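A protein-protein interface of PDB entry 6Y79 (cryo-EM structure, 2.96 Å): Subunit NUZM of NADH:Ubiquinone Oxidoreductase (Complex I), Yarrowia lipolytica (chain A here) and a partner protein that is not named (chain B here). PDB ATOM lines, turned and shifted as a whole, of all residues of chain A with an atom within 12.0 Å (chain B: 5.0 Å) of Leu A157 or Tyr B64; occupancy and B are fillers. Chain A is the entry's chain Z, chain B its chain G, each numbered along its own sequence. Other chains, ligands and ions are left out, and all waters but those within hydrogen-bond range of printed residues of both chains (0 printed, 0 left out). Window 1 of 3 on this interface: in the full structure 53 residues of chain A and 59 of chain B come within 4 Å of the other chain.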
ATOM      1  N   HIS A  79     -22.972  29.947  11.295  1.00  0.00           N
ATOM      2  CA  HIS A  79     -23.794  28.886  11.829  1.00  0.00           C
ATOM      3  C   HIS A  79     -24.140  29.102  13.289  1.00  0.00           C
ATOM      4  O   HIS A  79     -24.881  28.296  13.854  1.00  0.00           O
ATOM      5  CB  HIS A  79     -23.104  27.531  11.647  1.00  0.00           C
ATOM      6  CG  HIS A  79     -22.912  27.141  10.217  1.00  0.00           C
ATOM      7  ND1 HIS A  79     -23.970  26.910   9.366  1.00  0.00           N
ATOM      8  CD2 HIS A  79     -21.790  26.936   9.491  1.00  0.00           C
ATOM      9  CE1 HIS A  79     -23.507  26.586   8.173  1.00  0.00           C
ATOM     10  NE2 HIS A  79     -22.187  26.594   8.222  1.00  0.00           N
ATOM     11  N   ALA A  82     -27.604  30.297  12.818  1.00  0.00           N
ATOM     12  CA  ALA A  82     -28.426  29.259  12.213  1.00  0.00           C
ATOM     13  C   ALA A  82     -28.657  28.085  13.157  1.00  0.00           C
ATOM     14  O   ALA A  82     -28.780  26.943  12.709  1.00  0.00           O
ATOM     15  CB  ALA A  82     -27.795  28.774  10.910  1.00  0.00           C
ATOM     16  N   TYR A  83     -28.711  28.348  14.457  1.00  0.00           N
ATOM     17  CA  TYR A  83     -28.964  27.311  15.441  1.00  0.00           C
ATOM     18  C   TYR A  83     -30.408  26.819  15.347  1.00  0.00           C
ATOM     19  O   TYR A  83     -31.308  27.583  15.004  1.00  0.00           O
ATOM     20  CB  TYR A  83     -28.690  27.838  16.850  1.00  0.00           C
ATOM     21  CG  TYR A  83     -29.582  28.978  17.319  1.00  0.00           C
ATOM     22  CD1 TYR A  83     -29.332  30.284  16.927  1.00  0.00           C
ATOM     23  CD2 TYR A  83     -30.644  28.753  18.183  1.00  0.00           C
ATOM     24  CE1 TYR A  83     -30.119  31.321  17.353  1.00  0.00           C
ATOM     25  CE2 TYR A  83     -31.440  29.791  18.617  1.00  0.00           C
ATOM     26  CZ  TYR A  83     -31.169  31.074  18.198  1.00  0.00           C
ATOM     27  OH  TYR A  83     -31.951  32.122  18.624  1.00  0.00           O
ATOM     28  N   PRO A  84     -30.654  25.546  15.634  1.00  0.00           N
ATOM     29  CA  PRO A  84     -32.029  25.071  15.783  1.00  0.00           C
ATOM     30  C   PRO A  84     -32.546  25.264  17.202  1.00  0.00           C
ATOM     31  O   PRO A  84     -31.787  25.288  18.171  1.00  0.00           O
ATOM     32  CB  PRO A  84     -31.910  23.584  15.437  1.00  0.00           C
ATOM     33  CG  PRO A  84     -30.538  23.236  15.841  1.00  0.00           C
ATOM     34  CD  PRO A  84     -29.693  24.432  15.568  1.00  0.00           C
ATOM     35  N   GLN A  85     -33.864  25.420  17.319  1.00  0.00           N
ATOM     36  CA  GLN A  85     -34.429  25.532  18.661  1.00  0.00           C
ATOM     37  C   GLN A  85     -34.969  24.192  19.151  1.00  0.00           C
ATOM     38  O   GLN A  85     -35.159  23.245  18.387  1.00  0.00           O
ATOM     39  CB  GLN A  85     -35.546  26.591  18.761  1.00  0.00           C
ATOM     40  CG  GLN A  85     -36.917  26.207  18.199  1.00  0.00           C
ATOM     41  CD  GLN A  85     -37.048  26.567  16.711  1.00  0.00           C
ATOM     42  OE1 GLN A  85     -36.066  26.961  16.076  1.00  0.00           O
ATOM     43  NE2 GLN A  85     -38.245  26.395  16.166  1.00  0.00           N
ATOM     44  N   VAL A 153     -36.861   1.166  19.982  1.00  0.00           N
ATOM     45  CA  VAL A 153     -35.756   1.031  20.915  1.00  0.00           C
ATOM     46  C   VAL A 153     -35.108   2.396  21.105  1.00  0.00           C
ATOM     47  O   VAL A 153     -35.176   3.260  20.216  1.00  0.00           O
ATOM     48  CB  VAL A 153     -34.779  -0.049  20.407  1.00  0.00           C
ATOM     49  CG1 VAL A 153     -34.006   0.407  19.183  1.00  0.00           C
ATOM     50  CG2 VAL A 153     -33.850  -0.497  21.490  1.00  0.00           C
ATOM     51  N   ALA A 154     -34.555   2.629  22.308  1.00  0.00           N
ATOM     52  CA  ALA A 154     -33.878   3.862  22.701  1.00  0.00           C
ATOM     53  C   ALA A 154     -32.742   4.172  21.739  1.00  0.00           C
ATOM     54  O   ALA A 154     -31.763   3.418  21.663  1.00  0.00           O
ATOM     55  CB  ALA A 154     -33.349   3.759  24.129  1.00  0.00           C
ATOM     56  N   PRO A 155     -32.842   5.262  20.986  1.00  0.00           N
ATOM     57  CA  PRO A 155     -31.947   5.456  19.844  1.00  0.00           C
ATOM     58  C   PRO A 155     -30.563   5.920  20.266  1.00  0.00           C
ATOM     59  O   PRO A 155     -30.396   6.665  21.233  1.00  0.00           O
ATOM     60  CB  PRO A 155     -32.668   6.529  19.023  1.00  0.00           C
ATOM     61  CG  PRO A 155     -33.409   7.311  20.033  1.00  0.00           C
ATOM     62  CD  PRO A 155     -33.796   6.373  21.135  1.00  0.00           C
ATOM     63  N   THR A 156     -29.566   5.453  19.527  1.00  0.00           N
ATOM     64  CA  THR A 156     -28.200   5.925  19.654  1.00  0.00           C
ATOM     65  C   THR A 156     -27.764   6.505  18.317  1.00  0.00           C
ATOM     66  O   THR A 156     -28.302   6.150  17.264  1.00  0.00           O
ATOM     67  CB  THR A 156     -27.255   4.804  20.106  1.00  0.00           C
ATOM     68  OG1 THR A 156     -25.973   5.356  20.416  1.00  0.00           O
ATOM     69  CG2 THR A 156     -27.099   3.729  19.051  1.00  0.00           C
ATOM     70  N   LEU A 157     -26.822   7.444  18.369  1.00  0.00           N
ATOM     71  CA  LEU A 157     -26.388   8.129  17.160  1.00  0.00           C
ATOM     72  C   LEU A 157     -25.559   7.193  16.294  1.00  0.00           C
ATOM     73  O   LEU A 157     -25.953   6.855  15.174  1.00  0.00           O
ATOM     74  CB  LEU A 157     -25.583   9.378  17.513  1.00  0.00           C
ATOM     75  CG  LEU A 157     -25.317  10.421  16.426  1.00  0.00           C
ATOM     76  CD1 LEU A 157     -25.376  11.801  17.035  1.00  0.00           C
ATOM     77  CD2 LEU A 157     -23.969  10.217  15.760  1.00  0.00           C
ATOM     78  N   ALA A 158     -24.417   6.771  16.812  1.00  0.00           N
ATOM     79  CA  ALA A 158     -23.522   5.862  16.105  1.00  0.00           C
ATOM     80  C   ALA A 158     -23.421   4.574  16.900  1.00  0.00           C
ATOM     81  O   ALA A 158     -22.842   4.579  18.003  1.00  0.00           O
ATOM     82  CB  ALA A 158     -22.143   6.492  15.920  1.00  0.00           C
ATOM     83  N   PRO A 159     -23.978   3.465  16.417  1.00  0.00           N
ATOM     84  CA  PRO A 159     -23.878   2.211  17.166  1.00  0.00           C
ATOM     85  C   PRO A 159     -22.464   1.657  17.131  1.00  0.00           C
ATOM     86  O   PRO A 159     -21.748   1.787  16.137  1.00  0.00           O
ATOM     87  CB  PRO A 159     -24.859   1.287  16.439  1.00  0.00           C
ATOM     88  CG  PRO A 159     -24.931   1.838  15.060  1.00  0.00           C
ATOM     89  CD  PRO A 159     -24.792   3.321  15.200  1.00  0.00           C
ATOM     90  N   LYS A 160     -22.063   1.041  18.236  1.00  0.00           N
ATOM     91  CA  LYS A 160     -20.728   0.484  18.392  1.00  0.00           C
ATOM     92  C   LYS A 160     -20.832  -1.026  18.524  1.00  0.00           C
ATOM     93  O   LYS A 160     -21.376  -1.528  19.512  1.00  0.00           O
ATOM     94  CB  LYS A 160     -20.035   1.075  19.617  1.00  0.00           C
ATOM     95  CG  LYS A 160     -18.619   0.591  19.817  1.00  0.00           C
ATOM     96  CD  LYS A 160     -17.756   0.995  18.654  1.00  0.00           C
ATOM     97  CE  LYS A 160     -16.361   0.438  18.776  1.00  0.00           C
ATOM     98  NZ  LYS A 160     -15.518   0.909  17.648  1.00  0.00           N
ATOM     99  N   GLN A 161     -20.307  -1.746  17.539  1.00  0.00           N
ATOM    100  CA  GLN A 161     -20.235  -3.198  17.590  1.00  0.00           C
ATOM    101  C   GLN A 161     -18.849  -3.593  18.079  1.00  0.00           C
ATOM    102  O   GLN A 161     -17.842  -3.203  17.482  1.00  0.00           O
ATOM    103  CB  GLN A 161     -20.526  -3.815  16.225  1.00  0.00           C
ATOM    104  CG  GLN A 161     -21.953  -3.627  15.771  1.00  0.00           C
ATOM    105  CD  GLN A 161     -22.163  -4.063  14.342  1.00  0.00           C
ATOM    106  OE1 GLN A 161     -21.254  -4.594  13.705  1.00  0.00           O
ATOM    107  NE2 GLN A 161     -23.360  -3.825  13.820  1.00  0.00           N
ATOM    108  N   PRO B  60     -22.851  22.104  11.432  1.00  0.00           N
ATOM    109  CA  PRO B  60     -22.734  20.963  12.352  1.00  0.00           C
ATOM    110  C   PRO B  60     -24.054  20.351  12.768  1.00  0.00           C
ATOM    111  O   PRO B  60     -24.059  19.194  13.198  1.00  0.00           O
ATOM    112  CB  PRO B  60     -22.011  21.556  13.565  1.00  0.00           C
ATOM    113  CG  PRO B  60     -21.906  23.004  13.324  1.00  0.00           C
ATOM    114  CD  PRO B  60     -22.016  23.232  11.869  1.00  0.00           C
ATOM    115  N   ALA B  61     -25.168  21.068  12.657  1.00  0.00           N
ATOM    116  CA  ALA B  61     -26.445  20.483  13.013  1.00  0.00           C
ATOM    117  C   ALA B  61     -26.977  19.552  11.947  1.00  0.00           C
ATOM    118  O   ALA B  61     -27.934  18.856  12.225  1.00  0.00           O
ATOM    119  CB  ALA B  61     -27.482  21.568  13.294  1.00  0.00           C
ATOM    120  N   ASP B  62     -26.367  19.491  10.762  1.00  0.00           N
ATOM    121  CA  ASP B  62     -26.889  18.635   9.700  1.00  0.00           C
ATOM    122  C   ASP B  62     -26.570  17.165   9.930  1.00  0.00           C
ATOM    123  O   ASP B  62     -27.252  16.293   9.381  1.00  0.00           O
ATOM    124  CB  ASP B  62     -26.330  19.084   8.353  1.00  0.00           C
ATOM    125  CG  ASP B  62     -27.013  20.324   7.826  1.00  0.00           C
ATOM    126  OD1 ASP B  62     -27.927  20.838   8.507  1.00  0.00           O
ATOM    127  OD2 ASP B  62     -26.637  20.782   6.729  1.00  0.00           O
ATOM    128  N   ARG B  63     -25.535  16.866  10.715  1.00  0.00           N
ATOM    129  CA  ARG B  63     -25.176  15.475  10.955  1.00  0.00           C
ATOM    130  C   ARG B  63     -26.112  14.795  11.945  1.00  0.00           C
ATOM    131  O   ARG B  63     -26.133  13.563  12.013  1.00  0.00           O
ATOM    132  CB  ARG B  63     -23.738  15.380  11.456  1.00  0.00           C
ATOM    133  CG  ARG B  63     -23.537  15.961  12.829  1.00  0.00           C
ATOM    134  CD  ARG B  63     -22.110  15.802  13.286  1.00  0.00           C
ATOM    135  NE  ARG B  63     -21.782  14.401  13.498  1.00  0.00           N
ATOM    136  CZ  ARG B  63     -21.973  13.757  14.643  1.00  0.00           C
ATOM    137  NH1 ARG B  63     -22.485  14.392  15.687  1.00  0.00           N
ATOM    138  NH2 ARG B  63     -21.643  12.478  14.744  1.00  0.00           N
ATOM    139  N   TYR B  64     -26.892  15.562  12.699  1.00  0.00           N
ATOM    140  CA  TYR B  64     -27.734  15.009  13.747  1.00  0.00           C
ATOM    141  C   TYR B  64     -29.098  14.558  13.251  1.00  0.00           C
ATOM    142  O   TYR B  64     -29.687  13.665  13.872  1.00  0.00           O
ATOM    143  CB  TYR B  64     -27.941  16.044  14.852  1.00  0.00           C
ATOM    144  CG  TYR B  64     -26.689  16.408  15.599  1.00  0.00           C
ATOM    145  CD1 TYR B  64     -26.174  15.564  16.566  1.00  0.00           C
ATOM    146  CD2 TYR B  64     -26.026  17.603  15.348  1.00  0.00           C
ATOM    147  CE1 TYR B  64     -25.040  15.888  17.258  1.00  0.00           C
ATOM    148  CE2 TYR B  64     -24.879  17.935  16.042  1.00  0.00           C
ATOM    149  CZ  TYR B  64     -24.397  17.069  16.999  1.00  0.00           C
ATOM    150  OH  TYR B  64     -23.259  17.369  17.707  1.00  0.00           O
ATOM    151  N   LEU B  65     -29.539  15.088  12.097  1.00  0.00           N
ATOM    152  CA  LEU B  65     -30.960  15.250  11.763  1.00  0.00           C
ATOM    153  C   LEU B  65     -31.719  13.940  11.773  1.00  0.00           C
ATOM    154  O   LEU B  65     -32.795  13.845  12.383  1.00  0.00           O
ATOM    155  CB  LEU B  65     -31.112  15.887  10.382  1.00  0.00           C
ATOM    156  CG  LEU B  65     -30.468  17.258  10.211  1.00  0.00           C
ATOM    157  CD1 LEU B  65     -30.863  17.931   8.898  1.00  0.00           C
ATOM    158  CD2 LEU B  65     -30.837  18.117  11.385  1.00  0.00           C
ATOM    159  N   GLN B  66     -31.156  12.925  11.113  1.00  0.00           N
ATOM    160  CA  GLN B  66     -31.781  11.614  11.034  1.00  0.00           C
ATOM    161  C   GLN B  66     -31.989  11.021  12.418  1.00  0.00           C
ATOM    162  O   GLN B  66     -33.110  10.621  12.763  1.00  0.00           O
ATOM    163  CB  GLN B  66     -30.924  10.689  10.183  1.00  0.00           C
ATOM    164  CG  GLN B  66     -31.530   9.326  10.018  1.00  0.00           C
ATOM    165  CD  GLN B  66     -32.849   9.387   9.277  1.00  0.00           C
ATOM    166  OE1 GLN B  66     -32.985  10.099   8.279  1.00  0.00           O
ATOM    167  NE2 GLN B  66     -33.836   8.647   9.767  1.00  0.00           N
ATOM    168  N   HIS B  67     -30.943  11.049  13.252  1.00  0.00           N
ATOM    169  CA  HIS B  67     -31.086  10.578  14.622  1.00  0.00           C
ATOM    170  C   HIS B  67     -32.066  11.431  15.398  1.00  0.00           C
ATOM    171  O   HIS B  67     -32.846  10.892  16.194  1.00  0.00           O
ATOM    172  CB  HIS B  67     -29.744  10.562  15.343  1.00  0.00           C
ATOM    173  CG  HIS B  67     -29.839  10.071  16.751  1.00  0.00           C
ATOM    174  ND1 HIS B  67     -29.824  10.916  17.839  1.00  0.00           N
ATOM    175  CD2 HIS B  67     -29.985   8.822  17.247  1.00  0.00           C
ATOM    176  CE1 HIS B  67     -29.938  10.206  18.946  1.00  0.00           C
ATOM    177  NE2 HIS B  67     -30.038   8.933  18.615  1.00  0.00           N
ATOM    178  N   VAL B  68     -32.094  12.738  15.112  1.00  0.00           N
ATOM    179  CA  VAL B  68     -33.041  13.631  15.765  1.00  0.00           C
ATOM    180  C   VAL B  68     -34.465  13.225  15.416  1.00  0.00           C
ATOM    181  O   VAL B  68     -35.325  13.129  16.305  1.00  0.00           O
ATOM    182  CB  VAL B  68     -32.726  15.090  15.388  1.00  0.00           C
ATOM    183  CG1 VAL B  68     -33.789  16.021  15.869  1.00  0.00           C
ATOM    184  CG2 VAL B  68     -31.422  15.498  16.008  1.00  0.00           C
ATOM    185  N   LYS B  93     -31.584  18.785  19.774  1.00  0.00           N
ATOM    186  CA  LYS B  93     -30.586  18.293  18.849  1.00  0.00           C
ATOM    187  C   LYS B  93     -30.002  17.224  19.741  1.00  0.00           C
ATOM    188  O   LYS B  93     -29.875  17.500  20.941  1.00  0.00           O
ATOM    189  CB  LYS B  93     -29.582  19.371  18.470  1.00  0.00           C
ATOM    190  CG  LYS B  93     -28.352  18.904  17.765  1.00  0.00           C
ATOM    191  CD  LYS B  93     -27.208  19.886  17.977  1.00  0.00           C
ATOM    192  CE  LYS B  93     -27.544  21.261  17.458  1.00  0.00           C
ATOM    193  NZ  LYS B  93     -26.362  22.151  17.498  1.00  0.00           N
ATOM    194  N   ASP B  94     -29.948  15.982  19.233  1.00  0.00           N
ATOM    195  CA  ASP B  94     -29.482  14.737  19.869  1.00  0.00           C
ATOM    196  C   ASP B  94     -29.691  14.572  21.385  1.00  0.00           C
ATOM    197  O   ASP B  94     -28.930  13.857  22.040  1.00  0.00           O
ATOM    198  CB  ASP B  94     -28.002  14.485  19.542  1.00  0.00           C
ATOM    199  CG  ASP B  94     -26.973  15.371  20.307  1.00  0.00           C
ATOM    200  OD1 ASP B  94     -27.328  16.309  21.016  1.00  0.00           O
ATOM    201  OD2 ASP B  94     -25.771  15.035  20.211  1.00  0.00           O
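O of Pro A155 lies close to NE2 of His B67 (3.5 Å).
Lys B93 touches Pro A84. His B67 touches Thr A156. Leu A157 touches Arg B63 (CD2 to NH2, 3.4 Å). CD1 of Leu A157 touches CD1 of Tyr B64, at 3.9 Å. Leu A157 touches His B67 (N to NE2, 3.6 Å).
Leu A157 touches just these residues of chain B: Arg B63 (3.4 Å), Tyr B64 (3.9 Å) and His B67 (3.6 Å). Tyr B64 touches just one residue of chain A: Leu A157 (3.9 Å). No residue of chain A comes within 4 Å of Pro B60. No residue of chain A comes within 4 Å of Ala B61. Leu B65 touches none of the printed residues of chain A. Gln B66 touches none of the printed residues of chain A. Of chain A, only Pro A155, Thr A156 and Leu A157 come within 4 Å of His B67. No residue of chain A comes within 4 Å of Val B68. Asp B94 touches none of the printed residues of chain A. Of the printed residues of chain B, Thr A156 touches His B67 (3.2 Å). Printed residues of chain B within 4 Å of Pro A155: His B67. The nearest residue of chain B that does not touch Leu A157 is Asp B94 (4.5 Å). The nearest residue of chain A that does not touch Tyr B64 is Pro A84 (7.2 Å).
Of the 11 printed residues of chain B, 4 touch a printed residue of chain A. Printed residues of chain B that touch a printed residue of chain A: Arg B63, Tyr B64, His B67 and Lys B93. Of the 14 printed residues of chain A, 4 touch a printed residue of chain B. Among the printed residues, 6 pairs touch across the chains.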
